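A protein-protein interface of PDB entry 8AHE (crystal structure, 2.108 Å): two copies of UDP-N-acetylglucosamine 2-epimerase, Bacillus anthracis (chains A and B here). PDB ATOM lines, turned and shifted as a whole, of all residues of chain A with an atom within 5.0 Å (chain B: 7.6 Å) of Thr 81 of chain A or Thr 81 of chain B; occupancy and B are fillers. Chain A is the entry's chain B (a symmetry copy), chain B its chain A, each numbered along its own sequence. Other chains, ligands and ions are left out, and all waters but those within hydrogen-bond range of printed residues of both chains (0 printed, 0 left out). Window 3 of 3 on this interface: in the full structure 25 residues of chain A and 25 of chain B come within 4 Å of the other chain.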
ATOM      1  N   LEU A  76      -5.226 -19.314 -12.780  1.00  0.00           N
ATOM      2  CA  LEU A  76      -6.112 -20.469 -12.786  1.00  0.00           C
ATOM      3  C   LEU A  76      -5.328 -21.724 -12.408  1.00  0.00           C
ATOM      4  O   LEU A  76      -5.847 -22.595 -11.730  1.00  0.00           O
ATOM      5  CB  LEU A  76      -6.797 -20.598 -14.154  1.00  0.00           C
ATOM      6  CG  LEU A  76      -7.934 -19.616 -14.393  1.00  0.00           C
ATOM      7  CD1 LEU A  76      -8.537 -19.729 -15.783  1.00  0.00           C
ATOM      8  CD2 LEU A  76      -9.008 -19.863 -13.372  1.00  0.00           C
ATOM      9  N   ILE A  77      -4.096 -21.848 -12.907  1.00  0.00           N
ATOM     10  CA  ILE A  77      -3.271 -23.042 -12.766  1.00  0.00           C
ATOM     11  C   ILE A  77      -3.014 -23.312 -11.292  1.00  0.00           C
ATOM     12  O   ILE A  77      -3.152 -24.431 -10.859  1.00  0.00           O
ATOM     13  CB  ILE A  77      -1.936 -22.906 -13.533  1.00  0.00           C
ATOM     14  CG1 ILE A  77      -2.163 -23.079 -15.029  1.00  0.00           C
ATOM     15  CG2 ILE A  77      -0.889 -23.916 -13.046  1.00  0.00           C
ATOM     16  CD1 ILE A  77      -2.281 -24.521 -15.406  1.00  0.00           C
ATOM     17  N   ASP A  78      -2.612 -22.279 -10.558  1.00  0.00           N
ATOM     18  CA  ASP A  78      -2.246 -22.369  -9.151  1.00  0.00           C
ATOM     19  C   ASP A  78      -3.476 -22.697  -8.312  1.00  0.00           C
ATOM     20  O   ASP A  78      -3.419 -23.551  -7.448  1.00  0.00           O
ATOM     21  CB  ASP A  78      -1.564 -21.088  -8.656  1.00  0.00           C
ATOM     22  CG  ASP A  78      -0.159 -20.931  -9.229  1.00  0.00           C
ATOM     23  OD1 ASP A  78       0.478 -21.999  -9.533  1.00  0.00           O
ATOM     24  OD2 ASP A  78       0.288 -19.754  -9.406  1.00  0.00           O
ATOM     25  N   ILE A  79      -4.584 -22.023  -8.577  1.00  0.00           N
ATOM     26  CA  ILE A  79      -5.846 -22.281  -7.906  1.00  0.00           C
ATOM     27  C   ILE A  79      -6.260 -23.731  -8.136  1.00  0.00           C
ATOM     28  O   ILE A  79      -6.631 -24.396  -7.169  1.00  0.00           O
ATOM     29  CB  ILE A  79      -6.927 -21.278  -8.353  1.00  0.00           C
ATOM     30  CG1 ILE A  79      -6.525 -19.831  -7.981  1.00  0.00           C
ATOM     31  CG2 ILE A  79      -8.299 -21.657  -7.774  1.00  0.00           C
ATOM     32  CD1 ILE A  79      -7.411 -18.714  -8.639  1.00  0.00           C
ATOM     33  N   THR A  80      -6.145 -24.217  -9.402  1.00  0.00           N
ATOM     34  CA  THR A  80      -6.570 -25.536  -9.838  1.00  0.00           C
ATOM     35  C   THR A  80      -5.755 -26.631  -9.118  1.00  0.00           C
ATOM     36  O   THR A  80      -6.313 -27.558  -8.530  1.00  0.00           O
ATOM     37  CB  THR A  80      -6.559 -25.628 -11.366  1.00  0.00           C
ATOM     38  OG1 THR A  80      -7.460 -24.658 -11.925  1.00  0.00           O
ATOM     39  CG2 THR A  80      -6.942 -26.984 -11.894  1.00  0.00           C
ATOM     40  N   THR A  81      -4.428 -26.529  -9.144  1.00  0.00           N
ATOM     41  CA  THR A  81      -3.542 -27.499  -8.513  1.00  0.00           C
ATOM     42  C   THR A  81      -3.633 -27.484  -6.981  1.00  0.00           C
ATOM     43  O   THR A  81      -3.785 -28.559  -6.373  1.00  0.00           O
ATOM     44  CB  THR A  81      -2.090 -27.299  -8.961  1.00  0.00           C
ATOM     45  OG1 THR A  81      -1.616 -26.044  -8.464  1.00  0.00           O
ATOM     46  CG2 THR A  81      -1.957 -27.368 -10.460  1.00  0.00           C
ATOM     47  N   ARG A  82      -3.603 -26.294  -6.374  1.00  0.00           N
ATOM     48  CA  ARG A  82      -3.644 -26.170  -4.914  1.00  0.00           C
ATOM     49  C   ARG A  82      -5.036 -26.520  -4.364  1.00  0.00           C
ATOM     50  O   ARG A  82      -5.165 -27.203  -3.336  1.00  0.00           O
ATOM     51  CB  ARG A  82      -3.279 -24.754  -4.455  1.00  0.00           C
ATOM     52  CG  ARG A  82      -1.782 -24.444  -4.453  1.00  0.00           C
ATOM     53  CD  ARG A  82      -1.478 -23.280  -3.485  1.00  0.00           C
ATOM     54  NE  ARG A  82      -0.757 -22.159  -4.102  1.00  0.00           N
ATOM     55  CZ  ARG A  82      -1.334 -21.066  -4.635  1.00  0.00           C
ATOM     56  NH1 ARG A  82      -2.643 -20.863  -4.539  1.00  0.00           N
ATOM     57  NH2 ARG A  82      -0.589 -20.152  -5.240  1.00  0.00           N
ATOM     58  N   GLY A  83      -6.093 -26.073  -5.052  1.00  0.00           N
ATOM     59  CA  GLY A  83      -7.429 -26.500  -4.698  1.00  0.00           C
ATOM     60  C   GLY A  83      -7.642 -28.003  -4.846  1.00  0.00           C
ATOM     61  O   GLY A  83      -8.259 -28.570  -3.987  1.00  0.00           O
ATOM     62  N   LEU A  84      -7.167 -28.639  -5.948  1.00  0.00           N
ATOM     63  CA  LEU A  84      -7.293 -30.080  -6.135  1.00  0.00           C
ATOM     64  C   LEU A  84      -6.609 -30.873  -4.994  1.00  0.00           C
ATOM     65  O   LEU A  84      -7.241 -31.687  -4.323  1.00  0.00           O
ATOM     66  CB  LEU A  84      -6.678 -30.426  -7.476  1.00  0.00           C
ATOM     67  CG  LEU A  84      -6.788 -31.879  -7.900  1.00  0.00           C
ATOM     68  CD1 LEU A  84      -8.225 -32.320  -7.926  1.00  0.00           C
ATOM     69  CD2 LEU A  84      -6.138 -32.096  -9.261  1.00  0.00           C
ATOM     70  N   GLU A  85      -5.343 -30.576  -4.704  1.00  0.00           N
ATOM     71  CA  GLU A  85      -4.631 -31.104  -3.542  1.00  0.00           C
ATOM     72  C   GLU A  85      -5.436 -30.955  -2.254  1.00  0.00           C
ATOM     73  O   GLU A  85      -5.695 -31.958  -1.608  1.00  0.00           O
ATOM     74  CB  GLU A  85      -3.276 -30.417  -3.391  1.00  0.00           C
ATOM     75  CG  GLU A  85      -2.334 -30.817  -4.508  1.00  0.00           C
ATOM     76  CD  GLU A  85      -1.042 -30.024  -4.570  1.00  0.00           C
ATOM     77  OE1 GLU A  85      -0.925 -29.024  -3.853  1.00  0.00           O
ATOM     78  OE2 GLU A  85      -0.186 -30.413  -5.340  1.00  0.00           O
ATOM     79  N   THR B  75       0.452 -41.121  -8.327  1.00  0.00           N
ATOM     80  CA  THR B  75      -0.973 -40.957  -8.113  1.00  0.00           C
ATOM     81  C   THR B  75      -1.574 -40.112  -9.251  1.00  0.00           C
ATOM     82  O   THR B  75      -0.876 -39.294  -9.842  1.00  0.00           O
ATOM     83  CB  THR B  75      -1.138 -40.306  -6.728  1.00  0.00           C
ATOM     84  OG1 THR B  75      -0.555 -39.007  -6.763  1.00  0.00           O
ATOM     85  CG2 THR B  75      -0.405 -41.008  -5.599  1.00  0.00           C
ATOM     86  N   LEU B  76      -2.877 -40.305  -9.541  1.00  0.00           N
ATOM     87  CA  LEU B  76      -3.669 -39.434 -10.400  1.00  0.00           C
ATOM     88  C   LEU B  76      -3.464 -37.967 -10.065  1.00  0.00           C
ATOM     89  O   LEU B  76      -3.377 -37.172 -10.998  1.00  0.00           O
ATOM     90  CB  LEU B  76      -5.168 -39.751 -10.252  1.00  0.00           C
ATOM     91  CG  LEU B  76      -5.688 -40.831 -11.176  1.00  0.00           C
ATOM     92  CD1 LEU B  76      -7.159 -41.108 -10.887  1.00  0.00           C
ATOM     93  CD2 LEU B  76      -5.421 -40.443 -12.623  1.00  0.00           C
ATOM     94  N   ILE B  77      -3.528 -37.597  -8.764  1.00  0.00           N
ATOM     95  CA  ILE B  77      -3.372 -36.206  -8.338  1.00  0.00           C
ATOM     96  C   ILE B  77      -1.988 -35.733  -8.795  1.00  0.00           C
ATOM     97  O   ILE B  77      -1.897 -34.650  -9.396  1.00  0.00           O
ATOM     98  CB  ILE B  77      -3.504 -36.011  -6.810  1.00  0.00           C
ATOM     99  CG1 ILE B  77      -4.914 -36.287  -6.316  1.00  0.00           C
ATOM    100  CG2 ILE B  77      -3.091 -34.600  -6.400  1.00  0.00           C
ATOM    101  CD1 ILE B  77      -5.861 -35.135  -6.561  1.00  0.00           C
ATOM    102  N   ASP B  78      -0.914 -36.520  -8.513  1.00  0.00           N
ATOM    103  CA  ASP B  78       0.429 -36.010  -8.760  1.00  0.00           C
ATOM    104  C   ASP B  78       0.596 -35.811 -10.274  1.00  0.00           C
ATOM    105  O   ASP B  78       0.977 -34.732 -10.691  1.00  0.00           O
ATOM    106  CB  ASP B  78       1.531 -36.818  -8.064  1.00  0.00           C
ATOM    107  CG  ASP B  78       1.521 -36.775  -6.529  1.00  0.00           C
ATOM    108  OD1 ASP B  78       0.970 -35.816  -5.947  1.00  0.00           O
ATOM    109  OD2 ASP B  78       2.106 -37.714  -5.906  1.00  0.00           O
ATOM    110  N   ILE B  79       0.198 -36.799 -11.093  1.00  0.00           N
ATOM    111  CA  ILE B  79       0.319 -36.727 -12.547  1.00  0.00           C
ATOM    112  C   ILE B  79      -0.475 -35.548 -13.081  1.00  0.00           C
ATOM    113  O   ILE B  79      -0.030 -34.894 -14.014  1.00  0.00           O
ATOM    114  CB  ILE B  79      -0.149 -38.032 -13.244  1.00  0.00           C
ATOM    115  CG1 ILE B  79       0.621 -39.265 -12.729  1.00  0.00           C
ATOM    116  CG2 ILE B  79      -0.040 -37.869 -14.743  1.00  0.00           C
ATOM    117  CD1 ILE B  79      -0.040 -40.629 -12.991  1.00  0.00           C
ATOM    118  N   THR B  80      -1.645 -35.277 -12.469  1.00  0.00           N
ATOM    119  CA  THR B  80      -2.568 -34.214 -12.850  1.00  0.00           C
ATOM    120  C   THR B  80      -1.996 -32.818 -12.577  1.00  0.00           C
ATOM    121  O   THR B  80      -2.042 -31.971 -13.457  1.00  0.00           O
ATOM    122  CB  THR B  80      -3.914 -34.411 -12.132  1.00  0.00           C
ATOM    123  OG1 THR B  80      -4.551 -35.629 -12.571  1.00  0.00           O
ATOM    124  CG2 THR B  80      -4.846 -33.266 -12.379  1.00  0.00           C
ATOM    125  N   THR B  81      -1.453 -32.573 -11.373  1.00  0.00           N
ATOM    126  CA  THR B  81      -0.858 -31.285 -11.025  1.00  0.00           C
ATOM    127  C   THR B  81       0.464 -31.072 -11.772  1.00  0.00           C
ATOM    128  O   THR B  81       0.635 -30.045 -12.420  1.00  0.00           O
ATOM    129  CB  THR B  81      -0.706 -31.106  -9.516  1.00  0.00           C
ATOM    130  OG1 THR B  81       0.161 -32.113  -8.985  1.00  0.00           O
ATOM    131  CG2 THR B  81      -2.068 -31.140  -8.862  1.00  0.00           C
ATOM    132  N   ARG B  82       1.353 -32.063 -11.812  1.00  0.00           N
ATOM    133  CA  ARG B  82       2.645 -31.795 -12.432  1.00  0.00           C
ATOM    134  C   ARG B  82       2.445 -31.601 -13.933  1.00  0.00           C
ATOM    135  O   ARG B  82       3.035 -30.706 -14.555  1.00  0.00           O
ATOM    136  CB  ARG B  82       3.689 -32.872 -12.122  1.00  0.00           C
ATOM    137  CG  ARG B  82       3.811 -33.272 -10.651  1.00  0.00           C
ATOM    138  CD  ARG B  82       4.556 -34.592 -10.466  1.00  0.00           C
ATOM    139  NE  ARG B  82       5.987 -34.431 -10.714  1.00  0.00           N
ATOM    140  CZ  ARG B  82       6.886 -34.266  -9.752  1.00  0.00           C
ATOM    141  NH1 ARG B  82       7.937 -33.471  -9.955  1.00  0.00           N
ATOM    142  NH2 ARG B  82       6.637 -34.831  -8.576  1.00  0.00           N
ATOM    143  N   GLY B  83       1.625 -32.479 -14.530  1.00  0.00           N
ATOM    144  CA  GLY B  83       1.307 -32.425 -15.939  1.00  0.00           C
ATOM    145  C   GLY B  83       0.783 -31.053 -16.327  1.00  0.00           C
ATOM    146  O   GLY B  83       1.190 -30.463 -17.315  1.00  0.00           O
ATOM    147  N   LEU B  84      -0.177 -30.558 -15.556  1.00  0.00           N
ATOM    148  CA  LEU B  84      -0.852 -29.310 -15.887  1.00  0.00           C
ATOM    149  C   LEU B  84       0.117 -28.130 -15.827  1.00  0.00           C
ATOM    150  O   LEU B  84       0.109 -27.226 -16.693  1.00  0.00           O
ATOM    151  CB  LEU B  84      -2.021 -29.135 -14.906  1.00  0.00           C
ATOM    152  CG  LEU B  84      -2.891 -27.926 -15.169  1.00  0.00           C
ATOM    153  CD1 LEU B  84      -3.639 -28.098 -16.490  1.00  0.00           C
ATOM    154  CD2 LEU B  84      -3.787 -27.671 -13.988  1.00  0.00           C
ATOM    155  N   GLU B  85       0.968 -28.115 -14.800  1.00  0.00           N
ATOM    156  CA  GLU B  85       2.049 -27.127 -14.693  1.00  0.00           C
ATOM    157  C   GLU B  85       3.005 -27.161 -15.888  1.00  0.00           C
ATOM    158  O   GLU B  85       3.297 -26.114 -16.424  1.00  0.00           O
ATOM    159  CB  GLU B  85       2.836 -27.339 -13.407  1.00  0.00           C
ATOM    160  CG  GLU B  85       2.023 -27.010 -12.174  1.00  0.00           C
ATOM    161  CD  GLU B  85       2.694 -27.418 -10.863  1.00  0.00           C
ATOM    162  OE1 GLU B  85       3.765 -28.065 -10.895  1.00  0.00           O
ATOM    163  OE2 GLU B  85       2.130 -27.070  -9.825  1.00  0.00           O
ATOM    164  N   GLY B  86       3.478 -28.342 -16.276  1.00  0.00           N
ATOM    165  CA  GLY B  86       4.501 -28.504 -17.296  1.00  0.00           C
ATOM    166  C   GLY B  86       3.929 -28.232 -18.671  1.00  0.00           C
ATOM    167  O   GLY B  86       4.570 -27.511 -19.460  1.00  0.00           O
ATOM    168  N   LEU B  87       2.689 -28.704 -18.902  1.00  0.00           N
ATOM    169  CA  LEU B  87       1.992 -28.426 -20.159  1.00  0.00           C
ATOM    170  C   LEU B  87       1.620 -26.937 -20.310  1.00  0.00           C
ATOM    171  O   LEU B  87       1.778 -26.381 -21.403  1.00  0.00           O
ATOM    172  CB  LEU B  87       0.785 -29.360 -20.308  1.00  0.00           C
ATOM    173  CG  LEU B  87       1.143 -30.789 -20.698  1.00  0.00           C
ATOM    174  CD1 LEU B  87       0.076 -31.793 -20.287  1.00  0.00           C
ATOM    175  CD2 LEU B  87       1.396 -30.835 -22.190  1.00  0.00           C
ATOM    176  N   THR B 106      -4.939 -39.380 -19.040  1.00  0.00           N
ATOM    177  CA  THR B 106      -4.962 -38.258 -18.120  1.00  0.00           C
ATOM    178  C   THR B 106      -4.198 -37.072 -18.721  1.00  0.00           C
ATOM    179  O   THR B 106      -4.625 -35.943 -18.533  1.00  0.00           O
ATOM    180  CB  THR B 106      -4.501 -38.644 -16.708  1.00  0.00           C
ATOM    181  OG1 THR B 106      -5.560 -39.464 -16.199  1.00  0.00           O
ATOM    182  CG2 THR B 106      -4.366 -37.473 -15.755  1.00  0.00           C
ATOM    183  N   ILE B 110      -5.377 -33.097 -19.202  1.00  0.00           N
ATOM    184  CA  ILE B 110      -4.689 -31.947 -18.621  1.00  0.00           C
ATOM    185  C   ILE B 110      -4.060 -31.089 -19.692  1.00  0.00           C
ATOM    186  O   ILE B 110      -4.004 -29.864 -19.495  1.00  0.00           O
ATOM    187  CB  ILE B 110      -3.669 -32.320 -17.526  1.00  0.00           C
ATOM    188  CG1 ILE B 110      -2.567 -33.240 -18.011  1.00  0.00           C
ATOM    189  CG2 ILE B 110      -4.402 -32.882 -16.336  1.00  0.00           C
ATOM    190  CD1 ILE B 110      -1.916 -34.073 -16.878  1.00  0.00           C
ATOM    191  N   TYR B 117      -6.892 -22.949 -20.477  1.00  0.00           N
ATOM    192  CA  TYR B 117      -6.382 -21.900 -19.600  1.00  0.00           C
ATOM    193  C   TYR B 117      -5.485 -20.885 -20.322  1.00  0.00           C
ATOM    194  O   TYR B 117      -5.087 -19.878 -19.715  1.00  0.00           O
ATOM    195  CB  TYR B 117      -5.655 -22.514 -18.388  1.00  0.00           C
ATOM    196  CG  TYR B 117      -6.559 -23.075 -17.306  1.00  0.00           C
ATOM    197  CD1 TYR B 117      -7.948 -23.017 -17.374  1.00  0.00           C
ATOM    198  CD2 TYR B 117      -6.017 -23.704 -16.197  1.00  0.00           C
ATOM    199  CE1 TYR B 117      -8.769 -23.556 -16.376  1.00  0.00           C
ATOM    200  CE2 TYR B 117      -6.817 -24.267 -15.215  1.00  0.00           C
ATOM    201  CZ  TYR B 117      -8.188 -24.147 -15.273  1.00  0.00           C
ATOM    202  OH  TYR B 117      -8.926 -24.611 -14.232  1.00  0.00           O
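Ile 77 of chain A touches Leu 84 of chain B, and with the chains exchanged Leu 84 of chain A touches Ile 77 of chain B.
Thr 80 of chain A touches Leu 84 of chain B, and with the chains exchanged Leu 84 of chain A touches Thr 80 of chain B.
Thr 81 of chain A touches its own counterpart, Thr 81 of chain B.
Thr 81 of chain A touches Leu 84 of chain B, but with the chains exchanged Leu 84 of chain A does not touch Thr 81 of chain B (4.2 Å).
Of the 9 pairs that touch across the chains among the printed residues, 5 have their exchanged pair printed and touching as well.
Of the printed residues of chain B, Ile 77 of chain A touches Leu 84 and Tyr 117.
Of the printed residues of chain B, Thr 80 of chain A touches Leu 84 and Tyr 117.
Of the printed residues of chain B, Thr 81 of chain A touches Thr 81 (3.8 Å) and Leu 84 (3.99 Å).
Of the printed residues of chain B, Leu 84 of chain A touches Ile 77 and Thr 80.
Thr 81 of chain B touches just one residue of chain A: Thr 81.
Of the printed residues of chain A, Leu 84 of chain B touches Ile 77, Thr 80 and Thr 81.
Of the printed residues of chain A, Tyr 117 of chain B touches Leu 76, Ile 77 and Thr 80.
The nearest residue of chain A that does not touch Thr 81 of chain B is Glu 85 of chain A (4.04 Å).
The nearest printed residue of chain A that does not touch Ile 77 of chain B is Glu 85 of chain A (4.3 Å).
Along chain B the printed residues that touch a printed residue of chain A span positions 77 to 117.
Of the 10 printed residues of chain A, 5 touch a printed residue of chain B.
Hydrophobic or aromatic side chains of chain A within 4 Å of the printed part of chain B: Leu 76, Ile 77 and Leu 84.
Among the printed residues, 9 pairs touch across the chains.
Among the printed residues, no Asp or Glu carboxylate lies within 4 Å of a Lys or Arg side-chain nitrogen of the other chain.
Among the printed residues, merely in contact across the chains: Leu 76 of chain A with Tyr 117 of chain B, Ile 77 of chain A with Leu 84 of chain B, Ile 77 of chain A with Tyr 117 of chain B, Thr 80 of chain A with Leu 84 of chain B, Thr 81 of chain A with Thr 81 of chain B, Thr 81 of chain A with Leu 84 of chain B, Leu 84 of chain A with Ile 77 of chain B and Leu 84 of chain A with Thr 80 of chain B.
The side-chain hydroxyl (OH) of Tyr 117 of chain B sits at hydrogen-bond distance from the side-chain hydroxyl (OG1) of Thr 80 of chain A.
O of Leu 76 of chain B lies within hydrogen-bond range of OG1 of Thr 80 of chain B.
The backbone carbonyl oxygen of Ile 77 of chain B sits at hydrogen-bond distance from the side-chain hydroxyl of Thr 81 of chain B (3.3 Å).
The backbone carbonyl oxygen (O) of Asp 78 of chain B sits at hydrogen-bond distance from the side-chain hydroxyl (OG1) of Thr 81 of chain B, at 3.2 Å.
The backbone carbonyl oxygen (O) of Leu 76 of chain A lies within hydrogen-bond range of the side-chain hydroxyl (OG1) of Thr 80 of chain A (2.6 Å).
O of Ile 77 of chain A lies close to OG1 of Thr 81 of chain A, 3.3 Å away.
OG1 of Thr 81 of chain A sits at hydrogen-bond distance from O of Asp 78 of chain A.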
